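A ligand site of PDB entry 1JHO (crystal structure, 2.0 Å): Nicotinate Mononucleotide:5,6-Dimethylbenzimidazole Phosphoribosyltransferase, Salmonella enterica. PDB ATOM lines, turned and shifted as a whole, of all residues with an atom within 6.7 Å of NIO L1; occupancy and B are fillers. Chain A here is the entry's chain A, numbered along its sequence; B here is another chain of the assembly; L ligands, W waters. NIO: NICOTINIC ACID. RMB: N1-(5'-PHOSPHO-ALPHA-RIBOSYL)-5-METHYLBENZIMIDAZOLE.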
ATOM      1  N   GLU A 174      -4.492  17.338 -15.568  1.00  0.00           N
ATOM      2  CA  GLU A 174      -3.986  16.264 -16.419  1.00  0.00           C
ATOM      3  C   GLU A 174      -2.520  16.479 -16.770  1.00  0.00           C
ATOM      4  O   GLU A 174      -1.872  17.470 -16.433  1.00  0.00           O
ATOM      5  CB  GLU A 174      -4.811  16.170 -17.719  1.00  0.00           C
ATOM      6  CG  GLU A 174      -5.134  17.560 -18.343  1.00  0.00           C
ATOM      7  CD  GLU A 174      -3.885  18.379 -18.614  1.00  0.00           C
ATOM      8  OE1 GLU A 174      -3.023  18.062 -19.402  1.00  0.00           O
ATOM      9  OE2 GLU A 174      -3.822  19.455 -17.884  1.00  0.00           O
ATOM     10  N   ASN A 179      -2.236  15.970 -25.775  1.00  0.00           N
ATOM     11  CA  ASN A 179      -3.610  16.016 -25.287  1.00  0.00           C
ATOM     12  C   ASN A 179      -4.485  17.179 -25.737  1.00  0.00           C
ATOM     13  O   ASN A 179      -5.721  17.102 -25.668  1.00  0.00           O
ATOM     14  CB  ASN A 179      -3.820  15.601 -23.807  1.00  0.00           C
ATOM     15  CG  ASN A 179      -3.387  16.610 -22.760  1.00  0.00           C
ATOM     16  OD1 ASN A 179      -2.933  17.717 -23.081  1.00  0.00           O
ATOM     17  ND2 ASN A 179      -3.537  16.204 -21.497  1.00  0.00           N
ATOM     18  N   THR A 180      -3.875  18.273 -26.209  1.00  0.00           N
ATOM     19  CA  THR A 180      -4.724  19.380 -26.658  1.00  0.00           C
ATOM     20  C   THR A 180      -5.410  19.080 -27.996  1.00  0.00           C
ATOM     21  O   THR A 180      -6.350  19.760 -28.439  1.00  0.00           O
ATOM     22  CB  THR A 180      -3.998  20.742 -26.655  1.00  0.00           C
ATOM     23  OG1 THR A 180      -2.949  20.731 -27.605  1.00  0.00           O
ATOM     24  CG2 THR A 180      -3.415  21.004 -25.278  1.00  0.00           C
ATOM     25  N   ILE A 201      -2.139  26.306 -30.021  1.00  0.00           N
ATOM     26  CA  ILE A 201      -0.757  25.876 -30.053  1.00  0.00           C
ATOM     27  C   ILE A 201      -0.388  24.906 -28.945  1.00  0.00           C
ATOM     28  O   ILE A 201       0.765  24.477 -28.882  1.00  0.00           O
ATOM     29  CB  ILE A 201       0.253  27.015 -30.108  1.00  0.00           C
ATOM     30  CG1 ILE A 201       0.061  27.867 -28.864  1.00  0.00           C
ATOM     31  CG2 ILE A 201       0.055  27.845 -31.356  1.00  0.00           C
ATOM     32  CD1 ILE A 201       1.358  28.377 -28.263  1.00  0.00           C
ATOM     33  N   GLY A 202      -1.322  24.579 -28.063  1.00  0.00           N
ATOM     34  CA  GLY A 202      -0.962  23.631 -27.012  1.00  0.00           C
ATOM     35  C   GLY A 202       0.336  24.057 -26.329  1.00  0.00           C
ATOM     36  O   GLY A 202       0.538  25.219 -25.992  1.00  0.00           O
ATOM     37  N   ALA A 203       1.239  23.105 -26.141  1.00  0.00           N
ATOM     38  CA  ALA A 203       2.468  23.444 -25.477  1.00  0.00           C
ATOM     39  C   ALA A 203       3.539  23.943 -26.439  1.00  0.00           C
ATOM     40  O   ALA A 203       4.510  23.258 -26.750  1.00  0.00           O
ATOM     41  CB  ALA A 203       2.982  22.302 -24.602  1.00  0.00           C
ATOM     42  N   ASN A 204       3.340  25.172 -26.913  1.00  0.00           N
ATOM     43  CA  ASN A 204       4.299  25.781 -27.807  1.00  0.00           C
ATOM     44  C   ASN A 204       4.428  25.116 -29.158  1.00  0.00           C
ATOM     45  O   ASN A 204       5.523  25.007 -29.693  1.00  0.00           O
ATOM     46  CB  ASN A 204       5.671  26.023 -27.149  1.00  0.00           C
ATOM     47  CG  ASN A 204       5.560  26.991 -25.985  1.00  0.00           C
ATOM     48  OD1 ASN A 204       4.734  27.912 -26.021  1.00  0.00           O
ATOM     49  ND2 ASN A 204       6.369  26.779 -24.952  1.00  0.00           N
ATOM     50  N   ASP A 263      -9.995  23.500 -14.536  1.00  0.00           N
ATOM     51  CA  ASP A 263      -8.660  24.025 -14.766  1.00  0.00           C
ATOM     52  C   ASP A 263      -8.682  24.865 -16.048  1.00  0.00           C
ATOM     53  O   ASP A 263      -9.347  25.894 -16.096  1.00  0.00           O
ATOM     54  CB  ASP A 263      -7.557  22.932 -14.718  1.00  0.00           C
ATOM     55  CG  ASP A 263      -6.125  23.461 -14.813  1.00  0.00           C
ATOM     56  OD1 ASP A 263      -5.786  24.516 -14.356  1.00  0.00           O
ATOM     57  OD2 ASP A 263      -5.295  22.687 -15.448  1.00  0.00           O
ATOM     58  N   GLY A 264      -7.992  24.380 -17.086  1.00  0.00           N
ATOM     59  CA  GLY A 264      -7.912  25.037 -18.380  1.00  0.00           C
ATOM     60  C   GLY A 264      -8.660  24.335 -19.507  1.00  0.00           C
ATOM     61  O   GLY A 264      -9.689  23.678 -19.320  1.00  0.00           O
ATOM     62  N   PHE A 265      -8.107  24.487 -20.705  1.00  0.00           N
ATOM     63  CA  PHE A 265      -8.673  23.958 -21.919  1.00  0.00           C
ATOM     64  C   PHE A 265      -8.987  22.488 -21.883  1.00  0.00           C
ATOM     65  O   PHE A 265     -10.040  22.061 -22.322  1.00  0.00           O
ATOM     66  CB  PHE A 265      -7.756  24.271 -23.123  1.00  0.00           C
ATOM     67  CG  PHE A 265      -8.441  23.969 -24.439  1.00  0.00           C
ATOM     68  CD1 PHE A 265      -7.977  22.964 -25.303  1.00  0.00           C
ATOM     69  CD2 PHE A 265      -9.579  24.689 -24.795  1.00  0.00           C
ATOM     70  CE1 PHE A 265      -8.638  22.709 -26.506  1.00  0.00           C
ATOM     71  CE2 PHE A 265     -10.250  24.444 -26.001  1.00  0.00           C
ATOM     72  CZ  PHE A 265      -9.771  23.452 -26.844  1.00  0.00           C
ATOM     73  N   LEU A 266      -8.028  21.678 -21.419  1.00  0.00           N
ATOM     74  CA  LEU A 266      -8.275  20.255 -21.357  1.00  0.00           C
ATOM     75  C   LEU A 266      -9.504  20.006 -20.494  1.00  0.00           C
ATOM     76  O   LEU A 266     -10.364  19.196 -20.832  1.00  0.00           O
ATOM     77  CB  LEU A 266      -7.098  19.470 -20.754  1.00  0.00           C
ATOM     78  CG  LEU A 266      -5.839  19.422 -21.599  1.00  0.00           C
ATOM     79  CD1 LEU A 266      -6.182  19.232 -23.069  1.00  0.00           C
ATOM     80  CD2 LEU A 266      -5.002  20.675 -21.408  1.00  0.00           C
ATOM     81  N   SER A 267      -9.555  20.678 -19.335  1.00  0.00           N
ATOM     82  CA  SER A 267     -10.677  20.508 -18.416  1.00  0.00           C
ATOM     83  C   SER A 267     -11.995  20.956 -19.004  1.00  0.00           C
ATOM     84  O   SER A 267     -13.023  20.341 -18.707  1.00  0.00           O
ATOM     85  CB  SER A 267     -10.448  21.146 -17.052  1.00  0.00           C
ATOM     86  OG  SER A 267     -10.715  22.539 -17.131  1.00  0.00           O
ATOM     87  N   TYR A 268     -11.981  22.015 -19.808  1.00  0.00           N
ATOM     88  CA  TYR A 268     -13.241  22.447 -20.426  1.00  0.00           C
ATOM     89  C   TYR A 268     -13.806  21.317 -21.270  1.00  0.00           C
ATOM     90  O   TYR A 268     -14.992  21.051 -21.230  1.00  0.00           O
ATOM     91  CB  TYR A 268     -13.162  23.723 -21.275  1.00  0.00           C
ATOM     92  CG  TYR A 268     -12.414  24.883 -20.680  1.00  0.00           C
ATOM     93  CD1 TYR A 268     -11.811  25.800 -21.545  1.00  0.00           C
ATOM     94  CD2 TYR A 268     -12.301  25.088 -19.293  1.00  0.00           C
ATOM     95  CE1 TYR A 268     -11.088  26.899 -21.068  1.00  0.00           C
ATOM     96  CE2 TYR A 268     -11.593  26.189 -18.797  1.00  0.00           C
ATOM     97  CZ  TYR A 268     -10.989  27.076 -19.686  1.00  0.00           C
ATOM     98  OH  TYR A 268     -10.282  28.149 -19.236  1.00  0.00           O
ATOM     99  N   HIS A 289      -9.680  29.687 -14.175  1.00  0.00           N
ATOM    100  CA  HIS A 289      -9.070  30.708 -14.978  1.00  0.00           C
ATOM    101  C   HIS A 289      -9.449  30.610 -16.442  1.00  0.00           C
ATOM    102  O   HIS A 289     -10.038  29.631 -16.880  1.00  0.00           O
ATOM    103  CB  HIS A 289      -7.549  30.676 -14.804  1.00  0.00           C
ATOM    104  CG  HIS A 289      -6.904  29.607 -15.608  1.00  0.00           C
ATOM    105  ND1 HIS A 289      -7.201  28.261 -15.402  1.00  0.00           N
ATOM    106  CD2 HIS A 289      -5.990  29.700 -16.610  1.00  0.00           C
ATOM    107  CE1 HIS A 289      -6.458  27.571 -16.267  1.00  0.00           C
ATOM    108  NE2 HIS A 289      -5.730  28.407 -17.020  1.00  0.00           N
ATOM    109  N   SER A 291      -8.116  30.056 -19.834  1.00  0.00           N
ATOM    110  CA  SER A 291      -6.983  29.517 -20.581  1.00  0.00           C
ATOM    111  C   SER A 291      -6.635  30.317 -21.838  1.00  0.00           C
ATOM    112  O   SER A 291      -7.498  30.794 -22.580  1.00  0.00           O
ATOM    113  CB  SER A 291      -7.234  28.040 -20.898  1.00  0.00           C
ATOM    114  OG  SER A 291      -6.325  27.550 -21.879  1.00  0.00           O
ATOM    115  N   ALA A 292      -5.317  30.424 -22.101  1.00  0.00           N
ATOM    116  CA  ALA A 292      -4.805  31.121 -23.271  1.00  0.00           C
ATOM    117  C   ALA A 292      -4.923  30.306 -24.544  1.00  0.00           C
ATOM    118  O   ALA A 292      -4.490  30.758 -25.594  1.00  0.00           O
ATOM    119  CB  ALA A 292      -3.389  31.625 -23.057  1.00  0.00           C
ATOM    120  N   GLU A 293      -5.519  29.113 -24.452  1.00  0.00           N
ATOM    121  CA  GLU A 293      -5.726  28.287 -25.623  1.00  0.00           C
ATOM    122  C   GLU A 293      -6.803  28.931 -26.510  1.00  0.00           C
ATOM    123  O   GLU A 293      -7.842  29.391 -26.030  1.00  0.00           O
ATOM    124  CB  GLU A 293      -6.003  26.783 -25.281  1.00  0.00           C
ATOM    125  CG  GLU A 293      -6.107  25.885 -26.536  1.00  0.00           C
ATOM    126  CD  GLU A 293      -4.880  25.115 -26.988  1.00  0.00           C
ATOM    127  OE1 GLU A 293      -4.996  24.092 -27.606  1.00  0.00           O
ATOM    128  OE2 GLU A 293      -3.697  25.666 -26.716  1.00  0.00           O
ATOM    129  N   MET A 313      -2.809  31.808 -18.636  1.00  0.00           N
ATOM    130  CA  MET A 313      -2.147  30.561 -18.328  1.00  0.00           C
ATOM    131  C   MET A 313      -2.495  29.468 -19.328  1.00  0.00           C
ATOM    132  O   MET A 313      -3.607  29.421 -19.901  1.00  0.00           O
ATOM    133  CB  MET A 313      -2.382  30.141 -16.873  1.00  0.00           C
ATOM    134  CG  MET A 313      -1.586  30.976 -15.887  1.00  0.00           C
ATOM    135  SD  MET A 313      -2.157  30.761 -14.175  1.00  0.00           S
ATOM    136  CE  MET A 313      -2.286  28.956 -14.085  1.00  0.00           C
ATOM    137  N   ARG A 314      -1.516  28.593 -19.557  1.00  0.00           N
ATOM    138  CA  ARG A 314      -1.690  27.499 -20.503  1.00  0.00           C
ATOM    139  C   ARG A 314      -0.732  26.367 -20.168  1.00  0.00           C
ATOM    140  O   ARG A 314      -0.098  25.784 -21.037  1.00  0.00           O
ATOM    141  CB  ARG A 314      -1.501  27.992 -21.944  1.00  0.00           C
ATOM    142  CG  ARG A 314      -0.226  28.814 -22.087  1.00  0.00           C
ATOM    143  CD  ARG A 314      -0.019  29.331 -23.514  1.00  0.00           C
ATOM    144  NE  ARG A 314       1.213  30.112 -23.701  1.00  0.00           N
ATOM    145  CZ  ARG A 314       2.439  29.624 -23.935  1.00  0.00           C
ATOM    146  NH1 ARG A 314       2.690  28.315 -23.978  1.00  0.00           N
ATOM    147  NH2 ARG A 314       3.450  30.467 -24.110  1.00  0.00           N
ATOM    148  N   LEU A 315      -0.624  26.044 -18.887  1.00  0.00           N
ATOM    149  CA  LEU A 315       0.235  24.968 -18.464  1.00  0.00           C
ATOM    150  C   LEU A 315      -0.517  23.648 -18.290  1.00  0.00           C
ATOM    151  O   LEU A 315       0.024  22.571 -18.556  1.00  0.00           O
ATOM    152  CB  LEU A 315       0.936  25.324 -17.134  1.00  0.00           C
ATOM    153  CG  LEU A 315       1.730  24.173 -16.461  1.00  0.00           C
ATOM    154  CD1 LEU A 315       2.828  23.639 -17.376  1.00  0.00           C
ATOM    155  CD2 LEU A 315       2.377  24.708 -15.175  1.00  0.00           C
ATOM    156  N   GLY A 316      -1.757  23.731 -17.763  1.00  0.00           N
ATOM    157  CA  GLY A 316      -2.519  22.547 -17.448  1.00  0.00           C
ATOM    158  C   GLY A 316      -2.061  22.022 -16.070  1.00  0.00           C
ATOM    159  O   GLY A 316      -1.590  22.826 -15.226  1.00  0.00           O
ATOM    160  N   GLU A 317      -2.180  20.699 -15.872  1.00  0.00           N
ATOM    161  CA  GLU A 317      -1.808  19.977 -14.641  1.00  0.00           C
ATOM    162  C   GLU A 317      -2.760  20.258 -13.461  1.00  0.00           C
ATOM    163  O   GLU A 317      -2.638  19.697 -12.373  1.00  0.00           O
ATOM    164  CB  GLU A 317      -0.368  20.334 -14.139  1.00  0.00           C
ATOM    165  CG  GLU A 317       0.741  20.362 -15.202  1.00  0.00           C
ATOM    166  CD  GLU A 317       2.082  20.606 -14.565  1.00  0.00           C
ATOM    167  OE1 GLU A 317       2.210  20.921 -13.393  1.00  0.00           O
ATOM    168  OE2 GLU A 317       3.104  20.441 -15.381  1.00  0.00           O
ATOM    169  N   GLY A 318      -3.702  21.165 -13.662  1.00  0.00           N
ATOM    170  CA  GLY A 318      -4.567  21.542 -12.571  1.00  0.00           C
ATOM    171  C   GLY A 318      -3.998  22.794 -11.888  1.00  0.00           C
ATOM    172  O   GLY A 318      -4.412  23.191 -10.805  1.00  0.00           O
ATOM    173  N   SER A 319      -3.018  23.440 -12.522  1.00  0.00           N
ATOM    174  CA  SER A 319      -2.402  24.646 -11.947  1.00  0.00           C
ATOM    175  C   SER A 319      -3.378  25.812 -11.706  1.00  0.00           C
ATOM    176  O   SER A 319      -3.321  26.476 -10.664  1.00  0.00           O
ATOM    177  CB  SER A 319      -1.174  25.077 -12.712  1.00  0.00           C
ATOM    178  OG  SER A 319      -1.477  25.114 -14.086  1.00  0.00           O
ATOM    179  N   PRO B  32       6.612  24.286 -20.162  1.00  0.00           N
ATOM    180  CA  PRO B  32       6.891  24.888 -21.446  1.00  0.00           C
ATOM    181  C   PRO B  32       7.122  26.384 -21.217  1.00  0.00           C
ATOM    182  O   PRO B  32       6.441  27.027 -20.419  1.00  0.00           O
ATOM    183  CB  PRO B  32       5.692  24.629 -22.368  1.00  0.00           C
ATOM    184  CG  PRO B  32       4.760  23.698 -21.591  1.00  0.00           C
ATOM    185  CD  PRO B  32       5.283  23.614 -20.167  1.00  0.00           C
HETATM  186  N   NIO L   1      -1.643  22.506 -21.864  1.00  0.00           N
HETATM  187  C1  NIO L   1      -2.677  22.851 -21.039  1.00  0.00           C
HETATM  188  C2  NIO L   1      -3.460  23.951 -21.379  1.00  0.00           C
HETATM  189  C3  NIO L   1      -3.214  24.698 -22.579  1.00  0.00           C
HETATM  190  C4  NIO L   1      -2.136  24.226 -23.335  1.00  0.00           C
HETATM  191  C5  NIO L   1      -1.307  23.164 -23.044  1.00  0.00           C
HETATM  192  C6  NIO L   1      -4.613  24.371 -20.475  1.00  0.00           C
HETATM  193  O1  NIO L   1      -5.320  25.369 -20.796  1.00  0.00           O
HETATM  194  O2  NIO L   1      -4.870  23.719 -19.405  1.00  0.00           O
HETATM  195  N3  RMB L   2       2.727  20.209 -17.918  1.00  0.00           N
HETATM  196  N1  RMB L   2       1.722  20.272 -19.947  1.00  0.00           N
HETATM  197  C2  RMB L   2       1.577  20.281 -18.601  1.00  0.00           C
HETATM  198  C7A RMB L   2       3.113  20.113 -20.118  1.00  0.00           C
HETATM  199  C3A RMB L   2       3.722  20.112 -18.869  1.00  0.00           C
HETATM  200  C4  RMB L   2       5.108  20.043 -18.735  1.00  0.00           C
HETATM  201  C5  RMB L   2       5.890  19.956 -19.882  1.00  0.00           C
HETATM  202  C6  RMB L   2       5.283  19.956 -21.167  1.00  0.00           C
HETATM  203  C7  RMB L   2       3.900  20.021 -21.292  1.00  0.00           C
HETATM  204  C8  RMB L   2       7.407  19.886 -19.746  1.00  0.00           C
HETATM  205  P   RMB L   2       0.321  19.524 -26.369  1.00  0.00           P
HETATM  206  O1P RMB L   2      -0.991  18.944 -26.783  1.00  0.00           O
HETATM  207  O2P RMB L   2       0.962  20.585 -27.203  1.00  0.00           O
HETATM  208  O3P RMB L   2       1.249  18.436 -25.946  1.00  0.00           O
HETATM  209  O5' RMB L   2       0.009  20.173 -24.925  1.00  0.00           O
HETATM  210  C5' RMB L   2      -0.579  19.396 -23.872  1.00  0.00           C
HETATM  211  C4' RMB L   2       0.493  18.982 -22.890  1.00  0.00           C
HETATM  212  O4' RMB L   2       1.151  20.160 -22.309  1.00  0.00           O
HETATM  213  C3' RMB L   2      -0.021  18.218 -21.701  1.00  0.00           C
HETATM  214  O3' RMB L   2       1.006  17.454 -21.050  1.00  0.00           O
HETATM  215  C2' RMB L   2      -0.467  19.416 -20.847  1.00  0.00           C
HETATM  216  O2' RMB L   2      -0.551  18.973 -19.477  1.00  0.00           O
HETATM  217  C1' RMB L   2       0.682  20.417 -21.004  1.00  0.00           C
HETATM  218  O   HOH W   1      -4.635  25.097 -17.053  1.00  0.00           O
HETATM  219  O   HOH W   2      -6.866  22.095 -18.580  1.00  0.00           O
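Water W1 lies within hydrogen-bond range of an oxygen (O2) of NIO L1 (2.7 Å), the side-chain carboxylate of Asp 263 (3.0 Å), the backbone NH of Gly 316 (3.3 Å), the backbone NH of Gly 264 (3.4 Å) and a ring nitrogen (NE2) of His 289 (3.5 Å).
CG2 of Thr 180 touches C5 of NIO L1, 3.8 Å away.
Gly 202 touches NIO L1.
CA of Gly 264 touches O2 of NIO L1 (3.5 Å).
Leu 266 touches NIO L1 (CD2 to C1, 3.2 Å).
OE2 of Glu 293 touches C4 of NIO L1, 3.99 Å away.
O of Arg 314 touches C4 of NIO L1, 3.4 Å away.
C of Leu 315 touches C1 of NIO L1 (3.6 Å).
Gly 316 touches NIO L1 (CA to O2, 3.3 Å).
Of the 25 residues printed, 10 come within 4 Å of NIO L1.
The nearest printed residue that does not touch NIO L1 is Ala 203 (4.01 Å).
The backbone NH of Ala 203 is in hydrogen-bond range of an oxygen (O2P) of RMB L2 (2.7 Å).
An oxygen (O1P) of RMB L2 sits at hydrogen-bond distance from the backbone NH (N) of Asn 179 (3.4 Å).
An oxygen (O1P) of RMB L2 is in hydrogen-bond range of the backbone NH (N) of Thr 180 (3.0 Å).
The side-chain carboxylate (OE1) of Glu 174 lies within hydrogen-bond range of an oxygen (O2') of RMB L2 (2.6 Å).
An oxygen (O1) of NIO L1 is in hydrogen-bond range of the side-chain hydroxyl of Ser 291 (2.6 Å).
A nitrogen (N3) of RMB L2 is in hydrogen-bond range of the side-chain carboxylate of Glu 317 (2.6 Å).
An oxygen (O1) of NIO L1 sits at hydrogen-bond distance from the backbone NH of Phe 265.
An oxygen (O1P) of RMB L2 is in hydrogen-bond range of the side-chain hydroxyl (OG1) of Thr 180 (2.8 Å).
The backbone NH (N) of Gly 202 lies within hydrogen-bond range of the side-chain carboxylate (OE2) of Glu 293.
OG of Ser 319 is in hydrogen-bond range of O of Gly 316.
The backbone carbonyl oxygen (O) of Gly 264 sits at hydrogen-bond distance from the side-chain hydroxyl (OG) of Ser 267 (2.7 Å).
The side-chain amide oxygen of Asn 204 is in hydrogen-bond range of the guanidinium group of Arg 314 (2.9 Å).
The side-chain hydroxyl (OG) of Ser 291 sits close to the backbone NH (N) of Glu 293 (3.1 Å).
N of Ser 291 sits at hydrogen-bond distance from OH of Tyr 268, 2.9 Å away.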
